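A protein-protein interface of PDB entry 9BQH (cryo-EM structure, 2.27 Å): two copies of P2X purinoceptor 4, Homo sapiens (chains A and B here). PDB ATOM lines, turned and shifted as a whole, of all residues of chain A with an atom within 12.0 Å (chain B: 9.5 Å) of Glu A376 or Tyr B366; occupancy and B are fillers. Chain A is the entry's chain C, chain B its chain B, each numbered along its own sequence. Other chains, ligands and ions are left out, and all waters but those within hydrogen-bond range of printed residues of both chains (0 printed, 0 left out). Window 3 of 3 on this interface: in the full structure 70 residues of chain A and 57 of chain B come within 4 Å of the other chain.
Printed residues of chain B within 4 Å of Tyr A374: Leu B22 (3.5 Å) and Arg B24 (3.6 Å).
Of chain B, only Val B21, Leu B22, Tyr B366, Tyr B367 and Lys B370 come within 4 Å of Val A375.
Glu A376 touches just these residues of chain B: Arg B24 and Tyr B366.
Printed residues of chain A within 4 Å of Leu B22: Tyr A372, Lys A373, Tyr A374 and Val A375.
Printed residues of chain A within 4 Å of Arg B24: Tyr A374 (3.6 Å) and Glu A376 (3.5 Å).
No residue of chain A comes within 4 Å of Leu B365.
Of chain A, only Val A375 and Glu A376 come within 4 Å of Tyr B366.
No residue of chain A comes within 4 Å of Glu B369.
Lys B370 touches just these residues of chain A: Lys A373 (3.8 Å) and Val A375 (3.7 Å).
The nearest residue of chain A that does not touch Tyr B366 is Lys A373 (6.0 Å).
OE2 of Glu B369 is in salt-bridge range of NZ of Lys B370 (3.9 Å).
Among the printed residues, pairs that only touch across the chains: Tyr A372 with Leu B22 (3.9 Å), Lys A373 with Val B21 (3.6 Å), Lys A373 with Lys B370 (3.8 Å), Tyr A374 with Leu B22 (3.5 Å), Tyr A374 with Arg B24 (3.6 Å), Val A375 with Val B21 (3.1 Å), Val A375 with Tyr B366 (3.8 Å), Val A375 with Tyr B367 (3.97 Å), Val A375 with Lys B370 (3.7 Å) and Glu A376 with Tyr B366 (3.5 Å).
N of Leu B22 is in hydrogen-bond range of O of Lys A373, 2.7 Å away.
O of Leu B22 sits at hydrogen-bond distance from N of Val A375 (3.0 Å).
OE2 of Glu A376 is in salt-bridge range of NH2 of Arg B24 (3.5 Å).
Positions printed for both chains: 368, 369 and 372.
Printed residues of chain B that touch a printed residue of chain A: Val B21, Leu B22, Arg B24, Tyr B366, Tyr B367 and Lys B370.
Hydrophobic or aromatic side chains of chain B that line the printed part of chain A: Val B21, Leu B22, Tyr B366 and Tyr B367.
Of the 7 printed residues of chain A, 5 touch a printed residue of chain B.
Along chain A the printed residues that touch a printed residue of chain B span positions 372 to 376.
Among the printed residues, 13 pairs touch across the chains.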
ATOM      1  N   ARG A 368      18.805 -18.317  41.143  1.00  0.00           N
ATOM      2  CA  ARG A 368      17.849 -18.064  40.071  1.00  0.00           C
ATOM      3  C   ARG A 368      17.616 -16.570  39.903  1.00  0.00           C
ATOM      4  O   ARG A 368      17.526 -16.068  38.779  1.00  0.00           O
ATOM      5  CB  ARG A 368      16.543 -18.810  40.371  1.00  0.00           C
ATOM      6  CG  ARG A 368      15.253 -18.256  39.736  1.00  0.00           C
ATOM      7  CD  ARG A 368      14.869 -18.969  38.445  1.00  0.00           C
ATOM      8  NE  ARG A 368      14.920 -20.421  38.561  1.00  0.00           N
ATOM      9  CZ  ARG A 368      14.631 -21.260  37.576  1.00  0.00           C
ATOM     10  NH1 ARG A 368      14.243 -20.824  36.389  1.00  0.00           N
ATOM     11  NH2 ARG A 368      14.735 -22.568  37.786  1.00  0.00           N
ATOM     12  N   GLU A 369      17.505 -15.844  41.017  1.00  0.00           N
ATOM     13  CA  GLU A 369      17.351 -14.396  40.946  1.00  0.00           C
ATOM     14  C   GLU A 369      18.598 -13.740  40.362  1.00  0.00           C
ATOM     15  O   GLU A 369      18.500 -12.783  39.586  1.00  0.00           O
ATOM     16  CB  GLU A 369      17.036 -13.847  42.340  1.00  0.00           C
ATOM     17  CG  GLU A 369      17.326 -12.363  42.559  1.00  0.00           C
ATOM     18  CD  GLU A 369      17.326 -11.990  44.028  1.00  0.00           C
ATOM     19  OE1 GLU A 369      16.527 -12.572  44.792  1.00  0.00           O
ATOM     20  OE2 GLU A 369      18.128 -11.117  44.421  1.00  0.00           O
ATOM     21  N   TYR A 372      18.844 -14.889  36.210  1.00  0.00           N
ATOM     22  CA  TYR A 372      17.799 -14.537  35.257  1.00  0.00           C
ATOM     23  C   TYR A 372      17.246 -13.153  35.565  1.00  0.00           C
ATOM     24  O   TYR A 372      17.001 -12.818  36.727  1.00  0.00           O
ATOM     25  CB  TYR A 372      16.669 -15.568  35.287  1.00  0.00           C
ATOM     26  CG  TYR A 372      17.062 -16.913  34.727  1.00  0.00           C
ATOM     27  CD1 TYR A 372      17.232 -17.093  33.365  1.00  0.00           C
ATOM     28  CD2 TYR A 372      17.263 -18.001  35.562  1.00  0.00           C
ATOM     29  CE1 TYR A 372      17.594 -18.315  32.847  1.00  0.00           C
ATOM     30  CE2 TYR A 372      17.626 -19.229  35.053  1.00  0.00           C
ATOM     31  CZ  TYR A 372      17.789 -19.381  33.696  1.00  0.00           C
ATOM     32  OH  TYR A 372      18.152 -20.602  33.182  1.00  0.00           O
ATOM     33  N   LYS A 373      17.054 -12.356  34.518  1.00  0.00           N
ATOM     34  CA  LYS A 373      16.457 -11.030  34.610  1.00  0.00           C
ATOM     35  C   LYS A 373      15.142 -11.047  33.843  1.00  0.00           C
ATOM     36  O   LYS A 373      15.118 -11.403  32.661  1.00  0.00           O
ATOM     37  CB  LYS A 373      17.405  -9.969  34.046  1.00  0.00           C
ATOM     38  CG  LYS A 373      16.794  -8.590  33.820  1.00  0.00           C
ATOM     39  CD  LYS A 373      17.304  -7.582  34.835  1.00  0.00           C
ATOM     40  CE  LYS A 373      16.826  -6.173  34.521  1.00  0.00           C
ATOM     41  NZ  LYS A 373      15.484  -6.146  33.876  1.00  0.00           N
ATOM     42  N   TYR A 374      14.060 -10.658  34.510  1.00  0.00           N
ATOM     43  CA  TYR A 374      12.742 -10.614  33.888  1.00  0.00           C
ATOM     44  C   TYR A 374      12.490  -9.210  33.352  1.00  0.00           C
ATOM     45  O   TYR A 374      12.523  -8.235  34.110  1.00  0.00           O
ATOM     46  CB  TYR A 374      11.657 -11.010  34.888  1.00  0.00           C
ATOM     47  CG  TYR A 374      11.688 -12.473  35.264  1.00  0.00           C
ATOM     48  CD1 TYR A 374      12.564 -12.941  36.233  1.00  0.00           C
ATOM     49  CD2 TYR A 374      10.848 -13.387  34.644  1.00  0.00           C
ATOM     50  CE1 TYR A 374      12.600 -14.277  36.578  1.00  0.00           C
ATOM     51  CE2 TYR A 374      10.877 -14.725  34.981  1.00  0.00           C
ATOM     52  CZ  TYR A 374      11.756 -15.164  35.950  1.00  0.00           C
ATOM     53  OH  TYR A 374      11.791 -16.497  36.292  1.00  0.00           O
ATOM     54  N   VAL A 375      12.239  -9.110  32.052  1.00  0.00           N
ATOM     55  CA  VAL A 375      11.999  -7.822  31.411  1.00  0.00           C
ATOM     56  C   VAL A 375      10.525  -7.474  31.561  1.00  0.00           C
ATOM     57  O   VAL A 375       9.651  -8.219  31.104  1.00  0.00           O
ATOM     58  CB  VAL A 375      12.414  -7.857  29.933  1.00  0.00           C
ATOM     59  CG1 VAL A 375      11.802  -6.692  29.171  1.00  0.00           C
ATOM     60  CG2 VAL A 375      13.920  -7.842  29.818  1.00  0.00           C
ATOM     61  N   GLU A 376      10.246  -6.342  32.199  1.00  0.00           N
ATOM     62  CA  GLU A 376       8.874  -5.930  32.470  1.00  0.00           C
ATOM     63  C   GLU A 376       8.680  -4.449  32.169  1.00  0.00           C
ATOM     64  O   GLU A 376       7.937  -4.084  31.258  1.00  0.00           O
ATOM     65  CB  GLU A 376       8.509  -6.223  33.925  1.00  0.00           C
ATOM     66  CG  GLU A 376       8.632  -7.692  34.310  1.00  0.00           C
ATOM     67  CD  GLU A 376       8.616  -7.908  35.810  1.00  0.00           C
ATOM     68  OE1 GLU A 376       8.365  -6.936  36.551  1.00  0.00           O
ATOM     69  OE2 GLU A 376       8.857  -9.052  36.247  1.00  0.00           O
ATOM     70  N   VAL B  21      18.419 -12.717  29.881  1.00  0.00           N
ATOM     71  CA  VAL B  21      17.260 -11.831  29.855  1.00  0.00           C
ATOM     72  C   VAL B  21      16.047 -12.653  29.452  1.00  0.00           C
ATOM     73  O   VAL B  21      16.070 -13.343  28.427  1.00  0.00           O
ATOM     74  CB  VAL B  21      17.470 -10.663  28.876  1.00  0.00           C
ATOM     75  CG1 VAL B  21      16.398  -9.612  29.064  1.00  0.00           C
ATOM     76  CG2 VAL B  21      18.830 -10.054  29.067  1.00  0.00           C
ATOM     77  N   LEU B  22      14.984 -12.579  30.249  1.00  0.00           N
ATOM     78  CA  LEU B  22      13.752 -13.321  29.999  1.00  0.00           C
ATOM     79  C   LEU B  22      12.692 -12.351  29.500  1.00  0.00           C
ATOM     80  O   LEU B  22      12.168 -11.544  30.273  1.00  0.00           O
ATOM     81  CB  LEU B  22      13.279 -14.039  31.262  1.00  0.00           C
ATOM     82  CG  LEU B  22      14.182 -15.146  31.806  1.00  0.00           C
ATOM     83  CD1 LEU B  22      13.507 -15.843  32.966  1.00  0.00           C
ATOM     84  CD2 LEU B  22      14.543 -16.145  30.724  1.00  0.00           C
ATOM     85  N   ILE B  23      12.372 -12.437  28.212  1.00  0.00           N
ATOM     86  CA  ILE B  23      11.359 -11.598  27.585  1.00  0.00           C
ATOM     87  C   ILE B  23      10.067 -12.393  27.494  1.00  0.00           C
ATOM     88  O   ILE B  23      10.052 -13.513  26.969  1.00  0.00           O
ATOM     89  CB  ILE B  23      11.816 -11.120  26.196  1.00  0.00           C
ATOM     90  CG1 ILE B  23      12.977 -10.134  26.331  1.00  0.00           C
ATOM     91  CG2 ILE B  23      10.665 -10.480  25.446  1.00  0.00           C
ATOM     92  CD1 ILE B  23      13.921 -10.138  25.157  1.00  0.00           C
ATOM     93  N   ARG B  24       8.983 -11.819  28.007  1.00  0.00           N
ATOM     94  CA  ARG B  24       7.683 -12.488  28.045  1.00  0.00           C
ATOM     95  C   ARG B  24       6.921 -12.138  26.773  1.00  0.00           C
ATOM     96  O   ARG B  24       6.322 -11.066  26.667  1.00  0.00           O
ATOM     97  CB  ARG B  24       6.906 -12.079  29.290  1.00  0.00           C
ATOM     98  CG  ARG B  24       7.158 -12.973  30.490  1.00  0.00           C
ATOM     99  CD  ARG B  24       6.147 -12.728  31.594  1.00  0.00           C
ATOM    100  NE  ARG B  24       6.758 -12.818  32.915  1.00  0.00           N
ATOM    101  CZ  ARG B  24       6.956 -11.796  33.738  1.00  0.00           C
ATOM    102  NH1 ARG B  24       6.603 -10.561  33.413  1.00  0.00           N
ATOM    103  NH2 ARG B  24       7.525 -12.017  34.920  1.00  0.00           N
ATOM    104  N   VAL B 357      13.412 -10.057  17.778  1.00  0.00           N
ATOM    105  CA  VAL B 357      13.185  -9.257  18.977  1.00  0.00           C
ATOM    106  C   VAL B 357      13.779  -7.865  18.818  1.00  0.00           C
ATOM    107  O   VAL B 357      13.226  -6.881  19.322  1.00  0.00           O
ATOM    108  CB  VAL B 357      13.765  -9.979  20.208  1.00  0.00           C
ATOM    109  CG1 VAL B 357      13.903  -9.020  21.377  1.00  0.00           C
ATOM    110  CG2 VAL B 357      12.893 -11.155  20.592  1.00  0.00           C
ATOM    111  N   LEU B 358      14.914  -7.756  18.131  1.00  0.00           N
ATOM    112  CA  LEU B 358      15.647  -6.500  18.081  1.00  0.00           C
ATOM    113  C   LEU B 358      15.319  -5.652  16.862  1.00  0.00           C
ATOM    114  O   LEU B 358      15.616  -4.452  16.872  1.00  0.00           O
ATOM    115  CB  LEU B 358      17.153  -6.775  18.105  1.00  0.00           C
ATOM    116  CG  LEU B 358      17.694  -7.450  19.366  1.00  0.00           C
ATOM    117  CD1 LEU B 358      19.095  -7.969  19.121  1.00  0.00           C
ATOM    118  CD2 LEU B 358      17.678  -6.500  20.550  1.00  0.00           C
ATOM    119  N   MET B 361      10.011  -5.728  16.116  1.00  0.00           N
ATOM    120  CA  MET B 361       9.144  -5.654  17.282  1.00  0.00           C
ATOM    121  C   MET B 361       8.797  -4.200  17.561  1.00  0.00           C
ATOM    122  O   MET B 361       9.546  -3.288  17.203  1.00  0.00           O
ATOM    123  CB  MET B 361       9.811  -6.276  18.514  1.00  0.00           C
ATOM    124  CG  MET B 361      10.042  -7.769  18.411  1.00  0.00           C
ATOM    125  SD  MET B 361       8.518  -8.700  18.186  1.00  0.00           S
ATOM    126  CE  MET B 361       7.729  -8.417  19.766  1.00  0.00           C
ATOM    127  N   LYS B 362       7.648  -3.992  18.207  1.00  0.00           N
ATOM    128  CA  LYS B 362       7.241  -2.638  18.562  1.00  0.00           C
ATOM    129  C   LYS B 362       8.115  -2.071  19.674  1.00  0.00           C
ATOM    130  O   LYS B 362       8.504  -0.899  19.630  1.00  0.00           O
ATOM    131  CB  LYS B 362       5.770  -2.625  18.978  1.00  0.00           C
ATOM    132  N   LYS B 363       8.437  -2.889  20.679  1.00  0.00           N
ATOM    133  CA  LYS B 363       9.266  -2.474  21.804  1.00  0.00           C
ATOM    134  C   LYS B 363      10.737  -2.816  21.605  1.00  0.00           C
ATOM    135  O   LYS B 363      11.460  -3.023  22.587  1.00  0.00           O
ATOM    136  CB  LYS B 363       8.749  -3.111  23.095  1.00  0.00           C
ATOM    137  CG  LYS B 363       7.448  -2.522  23.606  1.00  0.00           C
ATOM    138  CD  LYS B 363       6.712  -3.499  24.514  1.00  0.00           C
ATOM    139  CE  LYS B 363       7.204  -3.424  25.952  1.00  0.00           C
ATOM    140  NZ  LYS B 363       6.110  -3.678  26.928  1.00  0.00           N
ATOM    141  N   ARG B 364      11.203  -2.875  20.357  1.00  0.00           N
ATOM    142  CA  ARG B 364      12.557  -3.357  20.099  1.00  0.00           C
ATOM    143  C   ARG B 364      13.610  -2.512  20.802  1.00  0.00           C
ATOM    144  O   ARG B 364      14.649  -3.040  21.208  1.00  0.00           O
ATOM    145  CB  ARG B 364      12.821  -3.397  18.593  1.00  0.00           C
ATOM    146  CG  ARG B 364      12.594  -2.084  17.871  1.00  0.00           C
ATOM    147  CD  ARG B 364      13.083  -2.160  16.437  1.00  0.00           C
ATOM    148  NE  ARG B 364      12.999  -0.875  15.755  1.00  0.00           N
ATOM    149  CZ  ARG B 364      13.678  -0.558  14.662  1.00  0.00           C
ATOM    150  NH1 ARG B 364      14.514  -1.411  14.094  1.00  0.00           N
ATOM    151  NH2 ARG B 364      13.518   0.648  14.126  1.00  0.00           N
ATOM    152  N   LEU B 365      13.374  -1.206  20.955  1.00  0.00           N
ATOM    153  CA  LEU B 365      14.345  -0.363  21.644  1.00  0.00           C
ATOM    154  C   LEU B 365      14.448  -0.727  23.122  1.00  0.00           C
ATOM    155  O   LEU B 365      15.546  -0.742  23.690  1.00  0.00           O
ATOM    156  CB  LEU B 365      13.972   1.109  21.479  1.00  0.00           C
ATOM    157  CG  LEU B 365      13.779   1.594  20.041  1.00  0.00           C
ATOM    158  CD1 LEU B 365      13.480   3.084  20.017  1.00  0.00           C
ATOM    159  CD2 LEU B 365      15.003   1.282  19.191  1.00  0.00           C
ATOM    160  N   TYR B 366      13.313  -1.020  23.760  1.00  0.00           N
ATOM    161  CA  TYR B 366      13.337  -1.423  25.162  1.00  0.00           C
ATOM    162  C   TYR B 366      14.117  -2.720  25.346  1.00  0.00           C
ATOM    163  O   TYR B 366      14.920  -2.849  26.278  1.00  0.00           O
ATOM    164  CB  TYR B 366      11.904  -1.573  25.676  1.00  0.00           C
ATOM    165  CG  TYR B 366      11.793  -1.834  27.159  1.00  0.00           C
ATOM    166  CD1 TYR B 366      10.927  -2.801  27.648  1.00  0.00           C
ATOM    167  CD2 TYR B 366      12.544  -1.111  28.072  1.00  0.00           C
ATOM    168  CE1 TYR B 366      10.818  -3.044  28.999  1.00  0.00           C
ATOM    169  CE2 TYR B 366      12.442  -1.347  29.425  1.00  0.00           C
ATOM    170  CZ  TYR B 366      11.578  -2.315  29.884  1.00  0.00           C
ATOM    171  OH  TYR B 366      11.473  -2.553  31.235  1.00  0.00           O
ATOM    172  N   TYR B 367      13.901  -3.692  24.458  1.00  0.00           N
ATOM    173  CA  TYR B 367      14.637  -4.948  24.542  1.00  0.00           C
ATOM    174  C   TYR B 367      16.117  -4.740  24.247  1.00  0.00           C
ATOM    175  O   TYR B 367      16.973  -5.391  24.855  1.00  0.00           O
ATOM    176  CB  TYR B 367      14.036  -5.969  23.580  1.00  0.00           C
ATOM    177  CG  TYR B 367      12.573  -6.252  23.828  1.00  0.00           C
ATOM    178  CD1 TYR B 367      12.072  -6.335  25.118  1.00  0.00           C
ATOM    179  CD2 TYR B 367      11.697  -6.444  22.775  1.00  0.00           C
ATOM    180  CE1 TYR B 367      10.743  -6.595  25.348  1.00  0.00           C
ATOM    181  CE2 TYR B 367      10.364  -6.705  22.997  1.00  0.00           C
ATOM    182  CZ  TYR B 367       9.891  -6.780  24.285  1.00  0.00           C
ATOM    183  OH  TYR B 367       8.560  -7.042  24.512  1.00  0.00           O
ATOM    184  N   ARG B 368      16.436  -3.848  23.307  1.00  0.00           N
ATOM    185  CA  ARG B 368      17.832  -3.531  23.030  1.00  0.00           C
ATOM    186  C   ARG B 368      18.504  -2.947  24.264  1.00  0.00           C
ATOM    187  O   ARG B 368      19.656  -3.272  24.569  1.00  0.00           O
ATOM    188  CB  ARG B 368      17.905  -2.568  21.837  1.00  0.00           C
ATOM    189  CG  ARG B 368      19.152  -1.668  21.734  1.00  0.00           C
ATOM    190  CD  ARG B 368      20.219  -2.229  20.803  1.00  0.00           C
ATOM    191  NE  ARG B 368      19.680  -2.679  19.526  1.00  0.00           N
ATOM    192  CZ  ARG B 368      20.409  -3.206  18.551  1.00  0.00           C
ATOM    193  NH1 ARG B 368      21.720  -3.345  18.666  1.00  0.00           N
ATOM    194  NH2 ARG B 368      19.807  -3.605  17.436  1.00  0.00           N
ATOM    195  N   GLU B 369      17.799  -2.071  24.980  1.00  0.00           N
ATOM    196  CA  GLU B 369      18.342  -1.517  26.217  1.00  0.00           C
ATOM    197  C   GLU B 369      18.512  -2.601  27.274  1.00  0.00           C
ATOM    198  O   GLU B 369      19.496  -2.602  28.021  1.00  0.00           O
ATOM    199  CB  GLU B 369      17.431  -0.392  26.716  1.00  0.00           C
ATOM    200  CG  GLU B 369      17.547  -0.040  28.197  1.00  0.00           C
ATOM    201  CD  GLU B 369      16.389   0.810  28.678  1.00  0.00           C
ATOM    202  OE1 GLU B 369      15.898   1.647  27.891  1.00  0.00           O
ATOM    203  OE2 GLU B 369      15.966   0.640  29.841  1.00  0.00           O
ATOM    204  N   LYS B 370      17.558  -3.529  27.359  1.00  0.00           N
ATOM    205  CA  LYS B 370      17.622  -4.566  28.386  1.00  0.00           C
ATOM    206  C   LYS B 370      18.732  -5.575  28.105  1.00  0.00           C
ATOM    207  O   LYS B 370      19.326  -6.125  29.038  1.00  0.00           O
ATOM    208  CB  LYS B 370      16.274  -5.279  28.490  1.00  0.00           C
ATOM    209  CG  LYS B 370      15.172  -4.446  29.125  1.00  0.00           C
ATOM    210  CD  LYS B 370      15.460  -4.152  30.588  1.00  0.00           C
ATOM    211  CE  LYS B 370      15.813  -2.691  30.807  1.00  0.00           C
ATOM    212  NZ  LYS B 370      16.598  -2.487  32.055  1.00  0.00           N
ATOM    213  N   LYS B 371      19.017  -5.843  26.831  1.00  0.00           N
ATOM    214  CA  LYS B 371      19.942  -6.907  26.459  1.00  0.00           C
ATOM    215  C   LYS B 371      21.393  -6.448  26.420  1.00  0.00           C
ATOM    216  O   LYS B 371      22.284  -7.199  26.828  1.00  0.00           O
ATOM    217  CB  LYS B 371      19.551  -7.482  25.096  1.00  0.00           C
ATOM    218  CG  LYS B 371      20.594  -8.402  24.479  1.00  0.00           C
ATOM    219  CD  LYS B 371      20.014  -9.192  23.319  1.00  0.00           C
ATOM    220  CE  LYS B 371      21.077  -9.996  22.588  1.00  0.00           C
ATOM    221  NZ  LYS B 371      21.619 -11.109  23.405  1.00  0.00           N
ATOM    222  N   TYR B 372      21.656  -5.237  25.936  1.00  0.00           N
ATOM    223  CA  TYR B 372      23.016  -4.756  25.721  1.00  0.00           C
ATOM    224  C   TYR B 372      23.380  -3.714  26.769  1.00  0.00           C
ATOM    225  O   TYR B 372      22.577  -2.830  27.081  1.00  0.00           O
ATOM    226  CB  TYR B 372      23.165  -4.162  24.320  1.00  0.00           C
ATOM    227  CG  TYR B 372      23.097  -5.188  23.216  1.00  0.00           C
ATOM    228  CD1 TYR B 372      24.148  -6.062  22.992  1.00  0.00           C
ATOM    229  CD2 TYR B 372      21.981  -5.284  22.401  1.00  0.00           C
ATOM    230  CE1 TYR B 372      24.090  -7.003  21.991  1.00  0.00           C
ATOM    231  CE2 TYR B 372      21.915  -6.223  21.395  1.00  0.00           C
ATOM    232  CZ  TYR B 372      22.972  -7.080  21.195  1.00  0.00           C
ATOM    233  OH  TYR B 372      22.911  -8.019  20.194  1.00  0.00           O
